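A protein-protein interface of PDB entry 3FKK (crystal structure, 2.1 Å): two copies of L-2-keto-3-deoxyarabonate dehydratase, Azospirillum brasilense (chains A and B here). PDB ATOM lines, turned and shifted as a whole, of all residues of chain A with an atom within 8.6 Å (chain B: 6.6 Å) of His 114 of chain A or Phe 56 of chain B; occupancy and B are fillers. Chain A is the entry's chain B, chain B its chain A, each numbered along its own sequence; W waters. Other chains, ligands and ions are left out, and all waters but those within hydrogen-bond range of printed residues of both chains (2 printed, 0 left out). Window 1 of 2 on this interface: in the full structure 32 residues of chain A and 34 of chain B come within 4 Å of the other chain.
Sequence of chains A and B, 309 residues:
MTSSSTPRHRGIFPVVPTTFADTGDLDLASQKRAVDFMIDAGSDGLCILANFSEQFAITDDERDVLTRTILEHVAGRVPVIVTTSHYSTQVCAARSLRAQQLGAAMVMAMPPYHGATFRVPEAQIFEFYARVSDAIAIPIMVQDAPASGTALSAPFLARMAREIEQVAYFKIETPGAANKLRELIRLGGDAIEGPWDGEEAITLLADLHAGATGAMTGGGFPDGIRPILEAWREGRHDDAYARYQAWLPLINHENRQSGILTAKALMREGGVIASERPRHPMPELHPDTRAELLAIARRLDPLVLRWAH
Printed residues of chain B within 4 Å of Val 91 of chain A: Thr 59.
Pro 112 of chain A touches none of the printed residues of chain B.
His 114 of chain A touches four residues of chain B.
Printed residues of chain B within 4 Å of Ala 116 of chain A: Ala 147 (3.0 Å).
Gln 55 of chain B touches just one residue of chain A: His 114.
Of chain A, only His 86, Tyr 87, His 114 and Phe 118 come within 4 Å of Phe 56 of chain B.
Printed residues of chain A within 4 Å of Ile 58 of chain B: His 86 (3.6 Å).
Printed residues of chain A within 4 Å of Gly 115 of chain B: Tyr 113 (3.8 Å), Gly 115 (3.6 Å) and Ala 147 (3.6 Å).
Printed residues of chain A within 4 Å of Ile 260 of chain B: Phe 118 (3.4 Å).
The nearest printed residue of chain A that does not touch Ala 57 of chain B is His 86 of chain A (4.01 Å).
O of Ala 50 of chain B sits close to N of Gln 55 of chain B (3.5 Å).
The side-chain amide nitrogen (ND2) of Asn 51 of chain B sits close to the side-chain amide nitrogen (NE2) of Gln 55 of chain B (3.0 Å).
The side-chain amide oxygen (OE1) of Gln 55 of chain B sits at hydrogen-bond distance from the guanidinium group (NH1) of Arg 63 of chain B (2.9 Å).
The side-chain hydroxyl (OG) of Ser 88 of chain A sits at hydrogen-bond distance from the backbone NH (N) of Val 91 of chain A, 3.1 Å away.
The backbone carbonyl oxygen (O) of Gly 115 of chain A is in hydrogen-bond range of the guanidinium group (NH1) of Arg 119 of chain A (2.9 Å).
Water W2 bridges O of Phe 56 of chain B and N of Tyr 87 of chain A.
Water W1 bridges the side-chain hydroxyl of Tyr 113 of chain B (2.9 Å) and a ring nitrogen (NE2) of His 114 of chain A (3.2 Å).
Tyr 113 of chain A touches Gly 115 of chain B, and with the chains exchanged Gly 115 of chain A touches Tyr 113 of chain B.
Gly 115 of chain A touches its own counterpart, Gly 115 of chain B.
Gly 115 of chain A touches Ala 147 of chain B, and with the chains exchanged Ala 147 of chain A touches Gly 115 of chain B.
NE2 of Gln 55 of chain B lies within hydrogen-bond range of NE2 of His 114 of chain A (3.4 Å).
N of Ala 116 of chain A lies within hydrogen-bond range of O of Ala 147 of chain B (3.0 Å).
The backbone NH of Ala 147 of chain B lies close to the side-chain hydroxyl of Thr 117 of chain A (3.3 Å).
O of Phe 56 of chain B touches NE2 of His 86 of chain A (3.5 Å).
Met 282 of chain B touches Tyr 87 of chain A.
Ser 88 of chain A touches Ala 57 of chain B.
CG2 of Val 91 of chain A touches CG2 of Thr 59 of chain B, at 3.9 Å.
Gly 115 of chain B touches Tyr 113 of chain A (CA to CE1, 3.8 Å).
Phe 56 of chain B touches His 114 of chain A.
His 114 of chain A touches Tyr 113 of chain B (CE1 to OH, 3.7 Å).
Gly 115 of chain A touches Tyr 113 of chain B.
O of Ala 147 of chain B touches CA of Gly 115 of chain A, 3.5 Å away.
Asn 51 of chain B touches Phe 118 of chain A (CG to CE2, 3.5 Å).
Hydrophobic or aromatic side chains of chain A that line the printed part of chain B: His 86, Tyr 87, Val 91, Tyr 113, His 114, Ala 116 and Phe 118.
Of the 18 printed residues of chain B, 11 touch a printed residue of chain A.
Hydrophobic or aromatic side chains of chain B that line the printed part of chain A: Phe 56, Tyr 113, Ala 147, Ile 260 and Met 282.
Among the printed residues, no Asp or Glu carboxylate lies within 4 Å of a Lys or Arg side-chain nitrogen of the other chain.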
ATOM      1  N   SER A  85      24.562 -21.917 -12.229  1.00  0.00           N
ATOM      2  CA  SER A  85      23.486 -20.940 -12.110  1.00  0.00           C
ATOM      3  C   SER A  85      22.127 -21.528 -11.735  1.00  0.00           C
ATOM      4  O   SER A  85      21.738 -22.586 -12.221  1.00  0.00           O
ATOM      5  CB  SER A  85      23.333 -20.164 -13.422  1.00  0.00           C
ATOM      6  OG  SER A  85      24.552 -19.557 -13.811  1.00  0.00           O
ATOM      7  N   HIS A  86      21.424 -20.824 -10.856  1.00  0.00           N
ATOM      8  CA  HIS A  86      20.080 -21.199 -10.423  1.00  0.00           C
ATOM      9  C   HIS A  86      19.552 -20.063  -9.561  1.00  0.00           C
ATOM     10  O   HIS A  86      20.316 -19.426  -8.840  1.00  0.00           O
ATOM     11  CB  HIS A  86      20.068 -22.487  -9.606  1.00  0.00           C
ATOM     12  CG  HIS A  86      18.691 -23.026  -9.378  1.00  0.00           C
ATOM     13  ND1 HIS A  86      18.087 -23.918 -10.239  1.00  0.00           N
ATOM     14  CD2 HIS A  86      17.766 -22.737  -8.431  1.00  0.00           C
ATOM     15  CE1 HIS A  86      16.851 -24.152  -9.835  1.00  0.00           C
ATOM     16  NE2 HIS A  86      16.631 -23.447  -8.740  1.00  0.00           N
ATOM     17  N   TYR A  87      18.252 -19.804  -9.645  1.00  0.00           N
ATOM     18  CA  TYR A  87      17.647 -18.728  -8.868  1.00  0.00           C
ATOM     19  C   TYR A  87      17.825 -18.956  -7.371  1.00  0.00           C
ATOM     20  O   TYR A  87      18.257 -18.057  -6.649  1.00  0.00           O
ATOM     21  CB  TYR A  87      16.159 -18.596  -9.215  1.00  0.00           C
ATOM     22  CG  TYR A  87      15.454 -17.472  -8.485  1.00  0.00           C
ATOM     23  CD1 TYR A  87      14.989 -17.638  -7.176  1.00  0.00           C
ATOM     24  CD2 TYR A  87      15.284 -16.227  -9.088  1.00  0.00           C
ATOM     25  CE1 TYR A  87      14.375 -16.587  -6.489  1.00  0.00           C
ATOM     26  CE2 TYR A  87      14.673 -15.169  -8.411  1.00  0.00           C
ATOM     27  CZ  TYR A  87      14.223 -15.352  -7.117  1.00  0.00           C
ATOM     28  OH  TYR A  87      13.631 -14.302  -6.453  1.00  0.00           O
ATOM     29  N   SER A  88      17.507 -20.166  -6.916  1.00  0.00           N
ATOM     30  CA  SER A  88      17.616 -20.518  -5.504  1.00  0.00           C
ATOM     31  C   SER A  88      19.048 -20.555  -4.983  1.00  0.00           C
ATOM     32  O   SER A  88      19.894 -21.285  -5.505  1.00  0.00           O
ATOM     33  CB  SER A  88      16.961 -21.872  -5.252  1.00  0.00           C
ATOM     34  OG  SER A  88      17.313 -22.373  -3.975  1.00  0.00           O
ATOM     35  N   THR A  89      19.308 -19.776  -3.939  1.00  0.00           N
ATOM     36  CA  THR A  89      20.637 -19.722  -3.339  1.00  0.00           C
ATOM     37  C   THR A  89      21.078 -21.108  -2.861  1.00  0.00           C
ATOM     38  O   THR A  89      22.191 -21.553  -3.153  1.00  0.00           O
ATOM     39  CB  THR A  89      20.661 -18.758  -2.142  1.00  0.00           C
ATOM     40  OG1 THR A  89      20.347 -17.437  -2.595  1.00  0.00           O
ATOM     41  CG2 THR A  89      22.037 -18.754  -1.479  1.00  0.00           C
ATOM     42  N   VAL A  91      19.949 -24.028  -3.799  1.00  0.00           N
ATOM     43  CA  VAL A  91      20.125 -24.959  -4.910  1.00  0.00           C
ATOM     44  C   VAL A  91      21.477 -24.702  -5.580  1.00  0.00           C
ATOM     45  O   VAL A  91      22.228 -25.636  -5.856  1.00  0.00           O
ATOM     46  CB  VAL A  91      19.014 -24.809  -5.967  1.00  0.00           C
ATOM     47  CG1 VAL A  91      19.303 -25.730  -7.155  1.00  0.00           C
ATOM     48  CG2 VAL A  91      17.663 -25.157  -5.355  1.00  0.00           C
ATOM     49  N   PRO A 111      23.710 -14.062 -11.988  1.00  0.00           N
ATOM     50  CA  PRO A 111      23.075 -13.589 -10.758  1.00  0.00           C
ATOM     51  C   PRO A 111      21.658 -14.171 -10.765  1.00  0.00           C
ATOM     52  O   PRO A 111      21.098 -14.431 -11.830  1.00  0.00           O
ATOM     53  CB  PRO A 111      23.087 -12.074 -10.931  1.00  0.00           C
ATOM     54  CG  PRO A 111      22.906 -11.918 -12.414  1.00  0.00           C
ATOM     55  CD  PRO A 111      23.874 -12.962 -12.955  1.00  0.00           C
ATOM     56  N   PRO A 112      21.070 -14.398  -9.582  1.00  0.00           N
ATOM     57  CA  PRO A 112      19.714 -14.956  -9.523  1.00  0.00           C
ATOM     58  C   PRO A 112      18.673 -14.080 -10.229  1.00  0.00           C
ATOM     59  O   PRO A 112      18.619 -12.866 -10.011  1.00  0.00           O
ATOM     60  CB  PRO A 112      19.457 -15.075  -8.020  1.00  0.00           C
ATOM     61  CG  PRO A 112      20.273 -13.939  -7.451  1.00  0.00           C
ATOM     62  CD  PRO A 112      21.559 -14.054  -8.235  1.00  0.00           C
ATOM     63  N   TYR A 113      17.857 -14.711 -11.069  1.00  0.00           N
ATOM     64  CA  TYR A 113      16.804 -14.028 -11.821  1.00  0.00           C
ATOM     65  C   TYR A 113      15.967 -15.103 -12.510  1.00  0.00           C
ATOM     66  O   TYR A 113      16.341 -16.275 -12.522  1.00  0.00           O
ATOM     67  CB  TYR A 113      17.417 -13.139 -12.909  1.00  0.00           C
ATOM     68  CG  TYR A 113      17.858 -13.939 -14.125  1.00  0.00           C
ATOM     69  CD1 TYR A 113      17.010 -14.104 -15.221  1.00  0.00           C
ATOM     70  CD2 TYR A 113      19.091 -14.596 -14.143  1.00  0.00           C
ATOM     71  CE1 TYR A 113      17.379 -14.906 -16.307  1.00  0.00           C
ATOM     72  CE2 TYR A 113      19.469 -15.400 -15.219  1.00  0.00           C
ATOM     73  CZ  TYR A 113      18.610 -15.551 -16.296  1.00  0.00           C
ATOM     74  OH  TYR A 113      18.981 -16.341 -17.359  1.00  0.00           O
ATOM     75  N   HIS A 114      14.839 -14.705 -13.085  1.00  0.00           N
ATOM     76  CA  HIS A 114      14.012 -15.643 -13.831  1.00  0.00           C
ATOM     77  C   HIS A 114      13.232 -14.948 -14.937  1.00  0.00           C
ATOM     78  O   HIS A 114      12.521 -13.969 -14.694  1.00  0.00           O
ATOM     79  CB  HIS A 114      13.036 -16.402 -12.936  1.00  0.00           C
ATOM     80  CG  HIS A 114      12.168 -17.356 -13.698  1.00  0.00           C
ATOM     81  ND1 HIS A 114      10.875 -17.054 -14.069  1.00  0.00           N
ATOM     82  CD2 HIS A 114      12.441 -18.566 -14.241  1.00  0.00           C
ATOM     83  CE1 HIS A 114      10.390 -18.035 -14.809  1.00  0.00           C
ATOM     84  NE2 HIS A 114      11.320 -18.964 -14.930  1.00  0.00           N
ATOM     85  N   GLY A 115      13.367 -15.476 -16.151  1.00  0.00           N
ATOM     86  CA  GLY A 115      12.684 -14.902 -17.293  1.00  0.00           C
ATOM     87  C   GLY A 115      13.131 -13.470 -17.494  1.00  0.00           C
ATOM     88  O   GLY A 115      14.316 -13.159 -17.358  1.00  0.00           O
ATOM     89  N   ALA A 116      12.184 -12.597 -17.816  1.00  0.00           N
ATOM     90  CA  ALA A 116      12.481 -11.188 -18.023  1.00  0.00           C
ATOM     91  C   ALA A 116      11.669 -10.366 -17.028  1.00  0.00           C
ATOM     92  O   ALA A 116      11.635  -9.136 -17.098  1.00  0.00           O
ATOM     93  CB  ALA A 116      12.130 -10.787 -19.451  1.00  0.00           C
ATOM     94  N   THR A 117      11.029 -11.059 -16.090  1.00  0.00           N
ATOM     95  CA  THR A 117      10.192 -10.411 -15.085  1.00  0.00           C
ATOM     96  C   THR A 117      10.719 -10.510 -13.653  1.00  0.00           C
ATOM     97  O   THR A 117      10.504  -9.605 -12.849  1.00  0.00           O
ATOM     98  CB  THR A 117       8.758 -11.000 -15.113  1.00  0.00           C
ATOM     99  OG1 THR A 117       8.147 -10.715 -16.377  1.00  0.00           O
ATOM    100  CG2 THR A 117       7.908 -10.405 -13.999  1.00  0.00           C
ATOM    101  N   PHE A 118      11.409 -11.602 -13.333  1.00  0.00           N
ATOM    102  CA  PHE A 118      11.918 -11.799 -11.978  1.00  0.00           C
ATOM    103  C   PHE A 118      13.348 -11.325 -11.731  1.00  0.00           C
ATOM    104  O   PHE A 118      14.311 -11.891 -12.255  1.00  0.00           O
ATOM    105  CB  PHE A 118      11.779 -13.275 -11.589  1.00  0.00           C
ATOM    106  CG  PHE A 118      10.357 -13.763 -11.585  1.00  0.00           C
ATOM    107  CD1 PHE A 118       9.426 -13.230 -10.699  1.00  0.00           C
ATOM    108  CD2 PHE A 118       9.939 -14.734 -12.489  1.00  0.00           C
ATOM    109  CE1 PHE A 118       8.100 -13.654 -10.713  1.00  0.00           C
ATOM    110  CE2 PHE A 118       8.613 -15.164 -12.513  1.00  0.00           C
ATOM    111  CZ  PHE A 118       7.692 -14.623 -11.623  1.00  0.00           C
ATOM    112  N   ARG A 119      13.465 -10.277 -10.918  1.00  0.00           N
ATOM    113  CA  ARG A 119      14.754  -9.693 -10.555  1.00  0.00           C
ATOM    114  C   ARG A 119      14.949  -9.716  -9.042  1.00  0.00           C
ATOM    115  O   ARG A 119      13.996  -9.886  -8.281  1.00  0.00           O
ATOM    116  CB  ARG A 119      14.853  -8.251 -11.071  1.00  0.00           C
ATOM    117  CG  ARG A 119      15.467  -8.117 -12.467  1.00  0.00           C
ATOM    118  CD  ARG A 119      14.874  -9.128 -13.429  1.00  0.00           C
ATOM    119  NE  ARG A 119      15.411  -9.002 -14.779  1.00  0.00           N
ATOM    120  CZ  ARG A 119      15.238  -9.913 -15.731  1.00  0.00           C
ATOM    121  NH1 ARG A 119      14.549 -11.016 -15.476  1.00  0.00           N
ATOM    122  NH2 ARG A 119      15.749  -9.719 -16.938  1.00  0.00           N
ATOM    123  N   VAL A 120      16.194  -9.533  -8.615  1.00  0.00           N
ATOM    124  CA  VAL A 120      16.537  -9.545  -7.200  1.00  0.00           C
ATOM    125  C   VAL A 120      17.340  -8.303  -6.819  1.00  0.00           C
ATOM    126  O   VAL A 120      18.264  -7.914  -7.526  1.00  0.00           O
ATOM    127  CB  VAL A 120      17.367 -10.802  -6.864  1.00  0.00           C
ATOM    128  CG1 VAL A 120      17.762 -10.792  -5.406  1.00  0.00           C
ATOM    129  CG2 VAL A 120      16.562 -12.054  -7.190  1.00  0.00           C
ATOM    130  N   ALA A 147      21.435 -11.902 -20.712  1.00  0.00           N
ATOM    131  CA  ALA A 147      20.412 -12.919 -20.466  1.00  0.00           C
ATOM    132  C   ALA A 147      19.739 -12.789 -19.101  1.00  0.00           C
ATOM    133  O   ALA A 147      18.567 -13.128 -18.948  1.00  0.00           O
ATOM    134  CB  ALA A 147      21.011 -14.311 -20.619  1.00  0.00           C
ATOM    135  N   SER A 148      20.480 -12.300 -18.111  1.00  0.00           N
ATOM    136  CA  SER A 148      19.937 -12.133 -16.767  1.00  0.00           C
ATOM    137  C   SER A 148      19.089 -10.864 -16.678  1.00  0.00           C
ATOM    138  O   SER A 148      18.238 -10.736 -15.795  1.00  0.00           O
ATOM    139  CB  SER A 148      21.071 -12.047 -15.746  1.00  0.00           C
ATOM    140  OG  SER A 148      21.814 -10.852 -15.921  1.00  0.00           O
ATOM    141  N   GLY A 149      19.334  -9.930 -17.593  1.00  0.00           N
ATOM    142  CA  GLY A 149      18.603  -8.676 -17.595  1.00  0.00           C
ATOM    143  C   GLY A 149      18.806  -7.945 -16.281  1.00  0.00           C
ATOM    144  O   GLY A 149      18.062  -7.020 -15.952  1.00  0.00           O
ATOM    145  N   THR A 150      19.826  -8.360 -15.533  1.00  0.00           N
ATOM    146  CA  THR A 150      20.130  -7.768 -14.234  1.00  0.00           C
ATOM    147  C   THR A 150      21.358  -6.863 -14.288  1.00  0.00           C
ATOM    148  O   THR A 150      22.338  -7.158 -14.974  1.00  0.00           O
ATOM    149  CB  THR A 150      20.353  -8.874 -13.174  1.00  0.00           C
ATOM    150  OG1 THR A 150      19.181  -9.694 -13.094  1.00  0.00           O
ATOM    151  CG2 THR A 150      20.628  -8.265 -11.806  1.00  0.00           C
ATOM    152  N   LEU B  49       2.518 -25.155  -9.701  1.00  0.00           N
ATOM    153  CA  LEU B  49       3.859 -24.970 -10.233  1.00  0.00           C
ATOM    154  C   LEU B  49       3.989 -23.839 -11.247  1.00  0.00           C
ATOM    155  O   LEU B  49       4.760 -23.939 -12.198  1.00  0.00           O
ATOM    156  CB  LEU B  49       4.357 -26.290 -10.838  1.00  0.00           C
ATOM    157  CG  LEU B  49       4.363 -27.467  -9.856  1.00  0.00           C
ATOM    158  CD1 LEU B  49       4.849 -28.718 -10.557  1.00  0.00           C
ATOM    159  CD2 LEU B  49       5.263 -27.152  -8.671  1.00  0.00           C
ATOM    160  N   ALA B  50       3.232 -22.767 -11.034  1.00  0.00           N
ATOM    161  CA  ALA B  50       3.283 -21.605 -11.907  1.00  0.00           C
ATOM    162  C   ALA B  50       4.293 -20.629 -11.301  1.00  0.00           C
ATOM    163  O   ALA B  50       4.904 -20.917 -10.270  1.00  0.00           O
ATOM    164  CB  ALA B  50       1.903 -20.952 -12.002  1.00  0.00           C
ATOM    165  N   ASN B  51       4.468 -19.474 -11.926  1.00  0.00           N
ATOM    166  CA  ASN B  51       5.426 -18.510 -11.409  1.00  0.00           C
ATOM    167  C   ASN B  51       5.054 -18.008 -10.014  1.00  0.00           C
ATOM    168  O   ASN B  51       5.936 -17.730  -9.193  1.00  0.00           O
ATOM    169  CB  ASN B  51       5.595 -17.362 -12.408  1.00  0.00           C
ATOM    170  CG  ASN B  51       6.532 -17.731 -13.559  1.00  0.00           C
ATOM    171  OD1 ASN B  51       6.456 -17.164 -14.651  1.00  0.00           O
ATOM    172  ND2 ASN B  51       7.433 -18.677 -13.305  1.00  0.00           N
ATOM    173  N   PHE B  52       3.758 -17.914  -9.726  1.00  0.00           N
ATOM    174  CA  PHE B  52       3.340 -17.483  -8.399  1.00  0.00           C
ATOM    175  C   PHE B  52       3.484 -18.642  -7.412  1.00  0.00           C
ATOM    176  O   PHE B  52       3.171 -18.510  -6.231  1.00  0.00           O
ATOM    177  CB  PHE B  52       1.900 -16.958  -8.411  1.00  0.00           C
ATOM    178  CG  PHE B  52       1.807 -15.452  -8.355  1.00  0.00           C
ATOM    179  CD1 PHE B  52       0.918 -14.828  -7.483  1.00  0.00           C
ATOM    180  CD2 PHE B  52       2.621 -14.659  -9.164  1.00  0.00           C
ATOM    181  CE1 PHE B  52       0.840 -13.436  -7.414  1.00  0.00           C
ATOM    182  CE2 PHE B  52       2.554 -13.266  -9.105  1.00  0.00           C
ATOM    183  CZ  PHE B  52       1.662 -12.652  -8.229  1.00  0.00           C
ATOM    184  N   SER B  53       3.964 -19.778  -7.914  1.00  0.00           N
ATOM    185  CA  SER B  53       4.203 -20.953  -7.083  1.00  0.00           C
ATOM    186  C   SER B  53       5.706 -21.008  -6.811  1.00  0.00           C
ATOM    187  O   SER B  53       6.209 -21.979  -6.249  1.00  0.00           O
ATOM    188  CB  SER B  53       3.784 -22.234  -7.809  1.00  0.00           C
ATOM    189  OG  SER B  53       2.435 -22.181  -8.224  1.00  0.00           O
ATOM    190  N   GLU B  54       6.415 -19.957  -7.224  1.00  0.00           N
ATOM    191  CA  GLU B  54       7.863 -19.873  -7.052  1.00  0.00           C
ATOM    192  C   GLU B  54       8.540 -21.094  -7.681  1.00  0.00           C
ATOM    193  O   GLU B  54       9.548 -21.593  -7.176  1.00  0.00           O
ATOM    194  CB  GLU B  54       8.213 -19.777  -5.558  1.00  0.00           C
ATOM    195  CG  GLU B  54       7.767 -18.464  -4.904  1.00  0.00           C
ATOM    196  CD  GLU B  54       7.871 -18.475  -3.385  1.00  0.00           C
ATOM    197  OE1 GLU B  54       8.996 -18.528  -2.850  1.00  0.00           O
ATOM    198  OE2 GLU B  54       6.815 -18.428  -2.724  1.00  0.00           O
ATOM    199  N   GLN B  55       7.988 -21.564  -8.795  1.00  0.00           N
ATOM    200  CA  GLN B  55       8.532 -22.736  -9.469  1.00  0.00           C
ATOM    201  C   GLN B  55       9.987 -22.548  -9.905  1.00  0.00           C
ATOM    202  O   GLN B  55      10.743 -23.522 -10.009  1.00  0.00           O
ATOM    203  CB  GLN B  55       7.647 -23.113 -10.667  1.00  0.00           C
ATOM    204  CG  GLN B  55       7.610 -22.108 -11.814  1.00  0.00           C
ATOM    205  CD  GLN B  55       8.809 -22.231 -12.735  1.00  0.00           C
ATOM    206  OE1 GLN B  55       9.319 -23.330 -12.962  1.00  0.00           O
ATOM    207  NE2 GLN B  55       9.252 -21.105 -13.288  1.00  0.00           N
ATOM    208  N   PHE B  56      10.379 -21.298 -10.136  1.00  0.00           N
ATOM    209  CA  PHE B  56      11.744 -20.992 -10.543  1.00  0.00           C
ATOM    210  C   PHE B  56      12.755 -21.271  -9.428  1.00  0.00           C
ATOM    211  O   PHE B  56      13.957 -21.380  -9.687  1.00  0.00           O
ATOM    212  CB  PHE B  56      11.854 -19.522 -10.981  1.00  0.00           C
ATOM    213  CG  PHE B  56      11.173 -18.556 -10.052  1.00  0.00           C
ATOM    214  CD1 PHE B  56       9.850 -18.173 -10.274  1.00  0.00           C
ATOM    215  CD2 PHE B  56      11.843 -18.043  -8.946  1.00  0.00           C
ATOM    216  CE1 PHE B  56       9.205 -17.292  -9.406  1.00  0.00           C
ATOM    217  CE2 PHE B  56      11.212 -17.163  -8.069  1.00  0.00           C
ATOM    218  CZ  PHE B  56       9.886 -16.785  -8.298  1.00  0.00           C
ATOM    219  N   ALA B  57      12.271 -21.404  -8.195  1.00  0.00           N
ATOM    220  CA  ALA B  57      13.151 -21.651  -7.056  1.00  0.00           C
ATOM    221  C   ALA B  57      13.257 -23.114  -6.607  1.00  0.00           C
ATOM    222  O   ALA B  57      13.873 -23.404  -5.577  1.00  0.00           O
ATOM    223  CB  ALA B  57      12.725 -20.771  -5.868  1.00  0.00           C
ATOM    224  N   ILE B  58      12.672 -24.039  -7.362  1.00  0.00           N
ATOM    225  CA  ILE B  58      12.755 -25.445  -6.972  1.00  0.00           C
ATOM    226  C   ILE B  58      13.471 -26.293  -8.017  1.00  0.00           C
ATOM    227  O   ILE B  58      13.717 -25.842  -9.132  1.00  0.00           O
ATOM    228  CB  ILE B  58      11.359 -26.044  -6.711  1.00  0.00           C
ATOM    229  CG1 ILE B  58      10.550 -26.084  -8.009  1.00  0.00           C
ATOM    230  CG2 ILE B  58      10.639 -25.224  -5.641  1.00  0.00           C
ATOM    231  CD1 ILE B  58       9.173 -26.694  -7.856  1.00  0.00           C
ATOM    232  N   THR B  59      13.806 -27.522  -7.640  1.00  0.00           N
ATOM    233  CA  THR B  59      14.498 -28.452  -8.531  1.00  0.00           C
ATOM    234  C   THR B  59      13.483 -29.377  -9.206  1.00  0.00           C
ATOM    235  O   THR B  59      12.320 -29.428  -8.795  1.00  0.00           O
ATOM    236  CB  THR B  59      15.473 -29.337  -7.743  1.00  0.00           C
ATOM    237  OG1 THR B  59      14.723 -30.246  -6.931  1.00  0.00           O
ATOM    238  CG2 THR B  59      16.365 -28.483  -6.836  1.00  0.00           C
ATOM    239  N   ARG B  63       9.782 -30.603  -8.014  1.00  0.00           N
ATOM    240  CA  ARG B  63       8.645 -30.382  -8.897  1.00  0.00           C
ATOM    241  C   ARG B  63       7.795 -31.645  -8.997  1.00  0.00           C
ATOM    242  O   ARG B  63       6.568 -31.585  -8.932  1.00  0.00           O
ATOM    243  CB  ARG B  63       9.133 -29.980 -10.295  1.00  0.00           C
ATOM    244  CG  ARG B  63       8.087 -30.162 -11.382  1.00  0.00           C
ATOM    245  CD  ARG B  63       8.630 -29.871 -12.780  1.00  0.00           C
ATOM    246  NE  ARG B  63       8.447 -28.477 -13.170  1.00  0.00           N
ATOM    247  CZ  ARG B  63       9.171 -27.466 -12.705  1.00  0.00           C
ATOM    248  NH1 ARG B  63       8.924 -26.229 -13.116  1.00  0.00           N
ATOM    249  NH2 ARG B  63      10.147 -27.697 -11.840  1.00  0.00           N
ATOM    250  N   MET B 110       4.365 -21.978 -20.919  1.00  0.00           N
ATOM    251  CA  MET B 110       4.839 -20.716 -21.460  1.00  0.00           C
ATOM    252  C   MET B 110       5.474 -21.084 -22.791  1.00  0.00           C
ATOM    253  O   MET B 110       5.891 -22.228 -22.982  1.00  0.00           O
ATOM    254  CB  MET B 110       5.928 -20.132 -20.554  1.00  0.00           C
ATOM    255  CG  MET B 110       5.419 -19.323 -19.387  1.00  0.00           C
ATOM    256  SD  MET B 110       4.922 -17.697 -19.942  1.00  0.00           S
ATOM    257  CE  MET B 110       6.300 -16.720 -19.385  1.00  0.00           C
ATOM    258  N   TYR B 113      11.471 -20.439 -24.249  1.00  0.00           N
ATOM    259  CA  TYR B 113      12.337 -19.265 -24.192  1.00  0.00           C
ATOM    260  C   TYR B 113      13.279 -19.447 -23.006  1.00  0.00           C
ATOM    261  O   TYR B 113      13.132 -20.391 -22.229  1.00  0.00           O
ATOM    262  CB  TYR B 113      11.499 -18.002 -23.953  1.00  0.00           C
ATOM    263  CG  TYR B 113      11.143 -17.789 -22.490  1.00  0.00           C
ATOM    264  CD1 TYR B 113      11.957 -17.016 -21.657  1.00  0.00           C
ATOM    265  CD2 TYR B 113      10.028 -18.413 -21.925  1.00  0.00           C
ATOM    266  CE1 TYR B 113      11.672 -16.871 -20.298  1.00  0.00           C
ATOM    267  CE2 TYR B 113       9.734 -18.277 -20.568  1.00  0.00           C
ATOM    268  CZ  TYR B 113      10.559 -17.507 -19.761  1.00  0.00           C
ATOM    269  OH  TYR B 113      10.280 -17.386 -18.420  1.00  0.00           O
ATOM    270  N   GLY B 115      15.503 -16.743 -20.230  1.00  0.00           N
ATOM    271  CA  GLY B 115      15.999 -15.441 -19.826  1.00  0.00           C
ATOM    272  C   GLY B 115      15.335 -14.358 -20.650  1.00  0.00           C
ATOM    273  O   GLY B 115      14.127 -14.401 -20.889  1.00  0.00           O
ATOM    274  N   ALA B 147       6.856 -12.363 -18.899  1.00  0.00           N
ATOM    275  CA  ALA B 147       8.017 -13.084 -18.383  1.00  0.00           C
ATOM    276  C   ALA B 147       8.770 -13.823 -19.486  1.00  0.00           C
ATOM    277  O   ALA B 147       9.990 -13.992 -19.407  1.00  0.00           O
ATOM    278  CB  ALA B 147       7.582 -14.068 -17.303  1.00  0.00           C
ATOM    279  N   ILE B 260       3.898 -11.949  -5.412  1.00  0.00           N
ATOM    280  CA  ILE B 260       3.876 -13.397  -5.202  1.00  0.00           C
ATOM    281  C   ILE B 260       3.573 -13.834  -3.774  1.00  0.00           C
ATOM    282  O   ILE B 260       2.728 -14.702  -3.553  1.00  0.00           O
ATOM    283  CB  ILE B 260       5.223 -14.035  -5.615  1.00  0.00           C
ATOM    284  CG1 ILE B 260       5.432 -13.877  -7.123  1.00  0.00           C
ATOM    285  CG2 ILE B 260       5.244 -15.513  -5.232  1.00  0.00           C
ATOM    286  CD1 ILE B 260       6.773 -14.387  -7.620  1.00  0.00           C
ATOM    287  N   MET B 282      14.892 -14.509  -2.988  1.00  0.00           N
ATOM    288  CA  MET B 282      13.697 -13.688  -3.131  1.00  0.00           C
ATOM    289  C   MET B 282      13.509 -12.937  -1.818  1.00  0.00           C
ATOM    290  O   MET B 282      13.511 -13.542  -0.746  1.00  0.00           O
ATOM    291  CB  MET B 282      12.469 -14.546  -3.419  1.00  0.00           C
ATOM    292  CG  MET B 282      11.262 -13.722  -3.821  1.00  0.00           C
ATOM    293  SD  MET B 282       9.856 -14.709  -4.357  1.00  0.00           S
ATOM    294  CE  MET B 282       8.573 -13.915  -3.469  1.00  0.00           C
HETATM  295  O   HOH W   1       8.779 -19.332 -16.876  1.00  0.00           O
HETATM  296  O   HOH W   2      16.102 -20.942 -11.546  1.00  0.00           O
